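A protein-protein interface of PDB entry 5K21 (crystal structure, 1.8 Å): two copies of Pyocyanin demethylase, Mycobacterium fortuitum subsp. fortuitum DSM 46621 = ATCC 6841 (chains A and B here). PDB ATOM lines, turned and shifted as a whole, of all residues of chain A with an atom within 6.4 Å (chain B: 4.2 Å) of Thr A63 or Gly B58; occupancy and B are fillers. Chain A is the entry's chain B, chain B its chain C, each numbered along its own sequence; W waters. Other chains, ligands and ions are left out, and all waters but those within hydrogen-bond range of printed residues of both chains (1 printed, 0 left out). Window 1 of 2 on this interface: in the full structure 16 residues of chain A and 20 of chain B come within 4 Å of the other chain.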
ATOM      1  N   ASP A  35      21.640  -3.419  32.519  1.00  0.00           N
ATOM      2  CA  ASP A  35      20.824  -2.218  32.673  1.00  0.00           C
ATOM      3  C   ASP A  35      20.428  -1.740  31.283  1.00  0.00           C
ATOM      4  O   ASP A  35      20.920  -2.246  30.267  1.00  0.00           O
ATOM      5  CB  ASP A  35      21.550  -1.114  33.476  1.00  0.00           C
ATOM      6  CG  ASP A  35      22.739  -0.480  32.733  1.00  0.00           C
ATOM      7  OD1 ASP A  35      23.386  -1.173  31.940  1.00  0.00           O
ATOM      8  OD2 ASP A  35      23.034   0.730  32.964  1.00  0.00           O
ATOM      9  N   VAL A  36      19.512  -0.772  31.255  1.00  0.00           N
ATOM     10  CA  VAL A  36      19.092  -0.182  29.993  1.00  0.00           C
ATOM     11  C   VAL A  36      20.323   0.212  29.204  1.00  0.00           C
ATOM     12  O   VAL A  36      21.288   0.759  29.756  1.00  0.00           O
ATOM     13  CB  VAL A  36      18.162   1.023  30.239  1.00  0.00           C
ATOM     14  CG1 VAL A  36      18.836   2.078  31.087  1.00  0.00           C
ATOM     15  CG2 VAL A  36      17.711   1.616  28.921  1.00  0.00           C
ATOM     16  N   GLY A  37      20.319  -0.135  27.909  1.00  0.00           N
ATOM     17  CA  GLY A  37      21.387   0.236  27.006  1.00  0.00           C
ATOM     18  C   GLY A  37      22.389  -0.853  26.737  1.00  0.00           C
ATOM     19  O   GLY A  37      23.251  -0.680  25.868  1.00  0.00           O
ATOM     20  N   ASP A  38      22.330  -1.959  27.459  1.00  0.00           N
ATOM     21  CA  ASP A  38      23.205  -3.045  27.109  1.00  0.00           C
ATOM     22  C   ASP A  38      22.735  -3.635  25.791  1.00  0.00           C
ATOM     23  O   ASP A  38      21.614  -3.382  25.328  1.00  0.00           O
ATOM     24  CB  ASP A  38      23.250  -4.079  28.234  1.00  0.00           C
ATOM     25  CG  ASP A  38      23.939  -3.541  29.480  1.00  0.00           C
ATOM     26  OD1 ASP A  38      24.667  -2.538  29.365  1.00  0.00           O
ATOM     27  OD2 ASP A  38      23.797  -4.118  30.564  1.00  0.00           O
ATOM     28  N   PHE A  61      18.783  -5.034  21.931  1.00  0.00           N
ATOM     29  CA  PHE A  61      19.007  -3.844  22.748  1.00  0.00           C
ATOM     30  C   PHE A  61      18.135  -3.940  23.989  1.00  0.00           C
ATOM     31  O   PHE A  61      16.919  -4.114  23.871  1.00  0.00           O
ATOM     32  CB  PHE A  61      18.653  -2.581  21.964  1.00  0.00           C
ATOM     33  CG  PHE A  61      19.273  -2.523  20.601  1.00  0.00           C
ATOM     34  CD1 PHE A  61      18.641  -3.087  19.506  1.00  0.00           C
ATOM     35  CD2 PHE A  61      20.492  -1.915  20.419  1.00  0.00           C
ATOM     36  CE1 PHE A  61      19.246  -3.054  18.236  1.00  0.00           C
ATOM     37  CE2 PHE A  61      21.096  -1.869  19.169  1.00  0.00           C
ATOM     38  CZ  PHE A  61      20.463  -2.430  18.073  1.00  0.00           C
ATOM     39  N   PHE A  62      18.751  -3.816  25.166  1.00  0.00           N
ATOM     40  CA  PHE A  62      18.025  -3.856  26.432  1.00  0.00           C
ATOM     41  C   PHE A  62      17.369  -2.492  26.653  1.00  0.00           C
ATOM     42  O   PHE A  62      18.028  -1.507  26.992  1.00  0.00           O
ATOM     43  CB  PHE A  62      18.982  -4.256  27.553  1.00  0.00           C
ATOM     44  CG  PHE A  62      19.416  -5.695  27.481  1.00  0.00           C
ATOM     45  CD1 PHE A  62      20.379  -6.102  26.564  1.00  0.00           C
ATOM     46  CD2 PHE A  62      18.860  -6.647  28.324  1.00  0.00           C
ATOM     47  CE1 PHE A  62      20.776  -7.423  26.473  1.00  0.00           C
ATOM     48  CE2 PHE A  62      19.261  -7.982  28.247  1.00  0.00           C
ATOM     49  CZ  PHE A  62      20.225  -8.368  27.312  1.00  0.00           C
ATOM     50  N   THR A  63      16.058  -2.428  26.463  1.00  0.00           N
ATOM     51  CA  THR A  63      15.330  -1.173  26.561  1.00  0.00           C
ATOM     52  C   THR A  63      14.846  -0.900  27.969  1.00  0.00           C
ATOM     53  O   THR A  63      14.602   0.253  28.320  1.00  0.00           O
ATOM     54  CB  THR A  63      14.130  -1.199  25.601  1.00  0.00           C
ATOM     55  OG1 THR A  63      13.324  -2.343  25.890  1.00  0.00           O
ATOM     56  CG2 THR A  63      14.605  -1.286  24.167  1.00  0.00           C
ATOM     57  N   ASN A  64      14.707  -1.932  28.787  1.00  0.00           N
ATOM     58  CA  ASN A  64      14.188  -1.763  30.133  1.00  0.00           C
ATOM     59  C   ASN A  64      14.649  -2.965  30.938  1.00  0.00           C
ATOM     60  O   ASN A  64      14.466  -4.107  30.506  1.00  0.00           O
ATOM     61  CB  ASN A  64      12.661  -1.650  30.136  1.00  0.00           C
ATOM     62  CG  ASN A  64      12.129  -1.165  31.463  1.00  0.00           C
ATOM     63  OD1 ASN A  64      12.021  -1.928  32.409  1.00  0.00           O
ATOM     64  ND2 ASN A  64      11.873   0.127  31.561  1.00  0.00           N
ATOM     65  N   VAL A  65      15.295  -2.707  32.066  1.00  0.00           N
ATOM     66  CA  VAL A  65      15.797  -3.765  32.928  1.00  0.00           C
ATOM     67  C   VAL A  65      15.297  -3.498  34.338  1.00  0.00           C
ATOM     68  O   VAL A  65      15.594  -2.452  34.923  1.00  0.00           O
ATOM     69  CB  VAL A  65      17.334  -3.861  32.910  1.00  0.00           C
ATOM     70  CG1 VAL A  65      17.807  -4.975  33.859  1.00  0.00           C
ATOM     71  CG2 VAL A  65      17.848  -4.134  31.490  1.00  0.00           C
ATOM     72  N   PRO A  70      13.897  -8.193  32.148  1.00  0.00           N
ATOM     73  CA  PRO A  70      14.705  -7.428  31.194  1.00  0.00           C
ATOM     74  C   PRO A  70      14.105  -7.484  29.798  1.00  0.00           C
ATOM     75  O   PRO A  70      14.044  -8.556  29.193  1.00  0.00           O
ATOM     76  CB  PRO A  70      16.067  -8.125  31.256  1.00  0.00           C
ATOM     77  CG  PRO A  70      15.740  -9.548  31.574  1.00  0.00           C
ATOM     78  CD  PRO A  70      14.416  -9.560  32.322  1.00  0.00           C
ATOM     79  N   MET A  71      13.634  -6.346  29.297  1.00  0.00           N
ATOM     80  CA  MET A  71      13.030  -6.250  27.974  1.00  0.00           C
ATOM     81  C   MET A  71      14.094  -5.951  26.932  1.00  0.00           C
ATOM     82  O   MET A  71      14.958  -5.092  27.146  1.00  0.00           O
ATOM     83  CB  MET A  71      11.976  -5.141  27.934  1.00  0.00           C
ATOM     84  CG  MET A  71      10.721  -5.392  28.758  1.00  0.00           C
ATOM     85  SD  MET A  71       9.604  -6.602  28.031  1.00  0.00           S
ATOM     86  CE  MET A  71       9.228  -5.864  26.444  1.00  0.00           C
ATOM     87  N   THR A  72      14.024  -6.647  25.794  1.00  0.00           N
ATOM     88  CA  THR A  72      14.919  -6.380  24.678  1.00  0.00           C
ATOM     89  C   THR A  72      14.118  -6.108  23.425  1.00  0.00           C
ATOM     90  O   THR A  72      13.098  -6.765  23.156  1.00  0.00           O
ATOM     91  CB  THR A  72      15.892  -7.533  24.317  1.00  0.00           C
ATOM     92  OG1 THR A  72      15.166  -8.747  24.107  1.00  0.00           O
ATOM     93  CG2 THR A  72      16.967  -7.717  25.366  1.00  0.00           C
ATOM     94  N   TYR A  73      14.618  -5.146  22.663  1.00  0.00           N
ATOM     95  CA  TYR A  73      14.266  -4.967  21.269  1.00  0.00           C
ATOM     96  C   TYR A  73      15.285  -5.744  20.443  1.00  0.00           C
ATOM     97  O   TYR A  73      16.488  -5.473  20.532  1.00  0.00           O
ATOM     98  CB  TYR A  73      14.261  -3.484  20.913  1.00  0.00           C
ATOM     99  CG  TYR A  73      14.296  -3.229  19.436  1.00  0.00           C
ATOM    100  CD1 TYR A  73      13.390  -3.848  18.592  1.00  0.00           C
ATOM    101  CD2 TYR A  73      15.226  -2.364  18.881  1.00  0.00           C
ATOM    102  CE1 TYR A  73      13.421  -3.634  17.232  1.00  0.00           C
ATOM    103  CE2 TYR A  73      15.259  -2.137  17.514  1.00  0.00           C
ATOM    104  CZ  TYR A  73      14.348  -2.771  16.702  1.00  0.00           C
ATOM    105  OH  TYR A  73      14.361  -2.559  15.341  1.00  0.00           O
ATOM    106  N   LEU A  90       9.926  -7.207  20.636  1.00  0.00           N
ATOM    107  CA  LEU A  90      10.098  -6.430  21.860  1.00  0.00           C
ATOM    108  C   LEU A  90       9.491  -7.291  22.962  1.00  0.00           C
ATOM    109  O   LEU A  90       8.266  -7.321  23.133  1.00  0.00           O
ATOM    110  CB  LEU A  90       9.429  -5.066  21.768  1.00  0.00           C
ATOM    111  CG  LEU A  90       9.522  -4.225  23.049  1.00  0.00           C
ATOM    112  CD1 LEU A  90      10.963  -3.776  23.270  1.00  0.00           C
ATOM    113  CD2 LEU A  90       8.611  -3.013  22.995  1.00  0.00           C
ATOM    114  N   GLN B  23      13.035   4.132  31.313  1.00  0.00           N
ATOM    115  CA  GLN B  23      14.485   4.047  31.429  1.00  0.00           C
ATOM    116  C   GLN B  23      15.134   4.514  30.136  1.00  0.00           C
ATOM    117  O   GLN B  23      14.589   4.328  29.043  1.00  0.00           O
ATOM    118  CB  GLN B  23      14.931   2.627  31.751  1.00  0.00           C
ATOM    119  CG  GLN B  23      14.422   2.111  33.080  1.00  0.00           C
ATOM    120  CD  GLN B  23      14.877   0.693  33.377  1.00  0.00           C
ATOM    121  OE1 GLN B  23      15.667   0.105  32.633  1.00  0.00           O
ATOM    122  NE2 GLN B  23      14.367   0.130  34.463  1.00  0.00           N
ATOM    123  N   ILE B  41      19.251   4.354  23.991  1.00  0.00           N
ATOM    124  CA  ILE B  41      18.374   3.195  24.087  1.00  0.00           C
ATOM    125  C   ILE B  41      17.386   3.481  25.217  1.00  0.00           C
ATOM    126  O   ILE B  41      17.781   3.970  26.280  1.00  0.00           O
ATOM    127  CB  ILE B  41      19.179   1.907  24.333  1.00  0.00           C
ATOM    128  CG1 ILE B  41      20.100   1.635  23.132  1.00  0.00           C
ATOM    129  CG2 ILE B  41      18.247   0.722  24.526  1.00  0.00           C
ATOM    130  CD1 ILE B  41      21.162   0.577  23.384  1.00  0.00           C
ATOM    131  N   PHE B  42      16.100   3.219  24.975  1.00  0.00           N
ATOM    132  CA  PHE B  42      15.094   3.730  25.886  1.00  0.00           C
ATOM    133  C   PHE B  42      13.834   2.874  25.887  1.00  0.00           C
ATOM    134  O   PHE B  42      13.571   2.099  24.965  1.00  0.00           O
ATOM    135  CB  PHE B  42      14.728   5.179  25.522  1.00  0.00           C
ATOM    136  CG  PHE B  42      14.324   5.340  24.086  1.00  0.00           C
ATOM    137  CD1 PHE B  42      12.999   5.193  23.702  1.00  0.00           C
ATOM    138  CD2 PHE B  42      15.275   5.590  23.109  1.00  0.00           C
ATOM    139  CE1 PHE B  42      12.631   5.306  22.384  1.00  0.00           C
ATOM    140  CE2 PHE B  42      14.909   5.705  21.781  1.00  0.00           C
ATOM    141  CZ  PHE B  42      13.591   5.560  21.418  1.00  0.00           C
ATOM    142  N   SER B  43      13.044   3.075  26.943  1.00  0.00           N
ATOM    143  CA  SER B  43      11.705   2.525  27.085  1.00  0.00           C
ATOM    144  C   SER B  43      10.812   3.603  27.682  1.00  0.00           C
ATOM    145  O   SER B  43      11.280   4.490  28.406  1.00  0.00           O
ATOM    146  CB  SER B  43      11.695   1.288  27.973  1.00  0.00           C
ATOM    147  OG  SER B  43      12.325   1.537  29.221  1.00  0.00           O
ATOM    148  N   GLY B  57       9.781   0.438  23.300  1.00  0.00           N
ATOM    149  CA  GLY B  57      11.215   0.290  23.438  1.00  0.00           C
ATOM    150  C   GLY B  57      11.858   0.694  22.135  1.00  0.00           C
ATOM    151  O   GLY B  57      11.285   0.442  21.074  1.00  0.00           O
ATOM    152  N   GLY B  58      13.033   1.314  22.187  1.00  0.00           N
ATOM    153  CA  GLY B  58      13.635   1.772  20.952  1.00  0.00           C
ATOM    154  C   GLY B  58      15.106   2.086  21.114  1.00  0.00           C
ATOM    155  O   GLY B  58      15.668   2.044  22.214  1.00  0.00           O
ATOM    156  N   ALA B  59      15.710   2.429  19.981  1.00  0.00           N
ATOM    157  CA  ALA B  59      17.118   2.800  19.916  1.00  0.00           C
ATOM    158  C   ALA B  59      17.287   3.877  18.859  1.00  0.00           C
ATOM    159  O   ALA B  59      16.655   3.823  17.798  1.00  0.00           O
ATOM    160  CB  ALA B  59      18.002   1.597  19.587  1.00  0.00           C
ATOM    161  N   GLU B  75      14.710   3.472  15.706  1.00  0.00           N
ATOM    162  CA  GLU B  75      13.823   2.334  15.576  1.00  0.00           C
ATOM    163  C   GLU B  75      12.996   2.291  16.850  1.00  0.00           C
ATOM    164  O   GLU B  75      13.535   2.449  17.946  1.00  0.00           O
ATOM    165  CB  GLU B  75      14.627   1.033  15.407  1.00  0.00           C
ATOM    166  CG  GLU B  75      15.209   0.819  14.031  1.00  0.00           C
ATOM    167  CD  GLU B  75      14.190   0.280  13.026  1.00  0.00           C
ATOM    168  OE1 GLU B  75      12.991   0.151  13.379  1.00  0.00           O
ATOM    169  OE2 GLU B  75      14.593  -0.022  11.882  1.00  0.00           O
HETATM  170  O   HOH W   1      18.166  -0.288  33.748  1.00  0.00           O
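The side-chain amide nitrogen (ND2) of Asn A64 lies within hydrogen-bond range of the side-chain hydroxyl (OG) of Ser B43 (2.8 Å).
The side-chain hydroxyl of Ser B43 lies within hydrogen-bond range of the backbone carbonyl oxygen of Thr A63 (2.8 Å).
N of Val A65 is in hydrogen-bond range of OE1 of Gln B23, 2.9 Å away.
O of Asn A64 sits at hydrogen-bond distance from N of Met A71 (2.7 Å).
The backbone NH (N) of Thr A63 sits at hydrogen-bond distance from the backbone carbonyl oxygen (O) of Met A71, 3.0 Å away.
N of Gly B58 sits at hydrogen-bond distance from O of Phe B42, 2.9 Å away.
O of Tyr A73 sits at hydrogen-bond distance from N of Phe A61 (2.7 Å).
O of Gln B23 is in hydrogen-bond range of N of Ser B43, 2.9 Å away.
N of Gly A37 lies within hydrogen-bond range of O of Phe A62, at 2.8 Å.
OE1 of Gln B23 touches CB of Val A36 (3.6 Å).
Val A36 touches Ile B41.
Ile B41 touches Gly A37 (CD1 to O, 3.5 Å).
Phe A61 touches Ile B41.
Phe A62 touches Ile B41.
Thr A63 touches Gly B57 (CG2 to CA, 3.8 Å).
Thr A63 touches Gly B58 (CG2 to N, 3.6 Å).
Asn A64 touches Gln B23 (CA to OE1, 3.5 Å).
Tyr A73 touches Glu B75.
Leu A90 touches Gly B57 (CD2 to N, 3.7 Å).
Of the printed residues of chain B, Val A36 touches Gln B23 and Ile B41.
Of chain B, only Phe B42, Ser B43, Gly B57 and Gly B58 come within 4 Å of Thr A63.
Printed residues of chain A within 4 Å of Ile B41: Val A36 (3.5 Å), Gly A37 (3.5 Å), Phe A61 (3.9 Å) and Phe A62 (3.3 Å).
Of the printed residues of chain A, Ser B43 touches Thr A63 and Asn A64.
Of the printed residues of chain A, Gly B57 touches Thr A63 and Leu A90.
Of the printed residues of chain A, Glu B75 touches Tyr A73.
The nearest printed residue of chain B that does not touch Phe A62 is Phe B42 (5.5 Å).
Hydrophobic or aromatic side chains of chain B within 4 Å of the printed part of chain A: Ile B41.
Along chain B the printed residues that touch a printed residue of chain A span positions 23 to 75.
Of the 14 printed residues of chain A, 9 touch a printed residue of chain B.
No position is printed for both chains.
Water W1 lies within hydrogen-bond range of OE1 of Gln B23 (2.8 Å) and N of Val A36 (2.9 Å).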
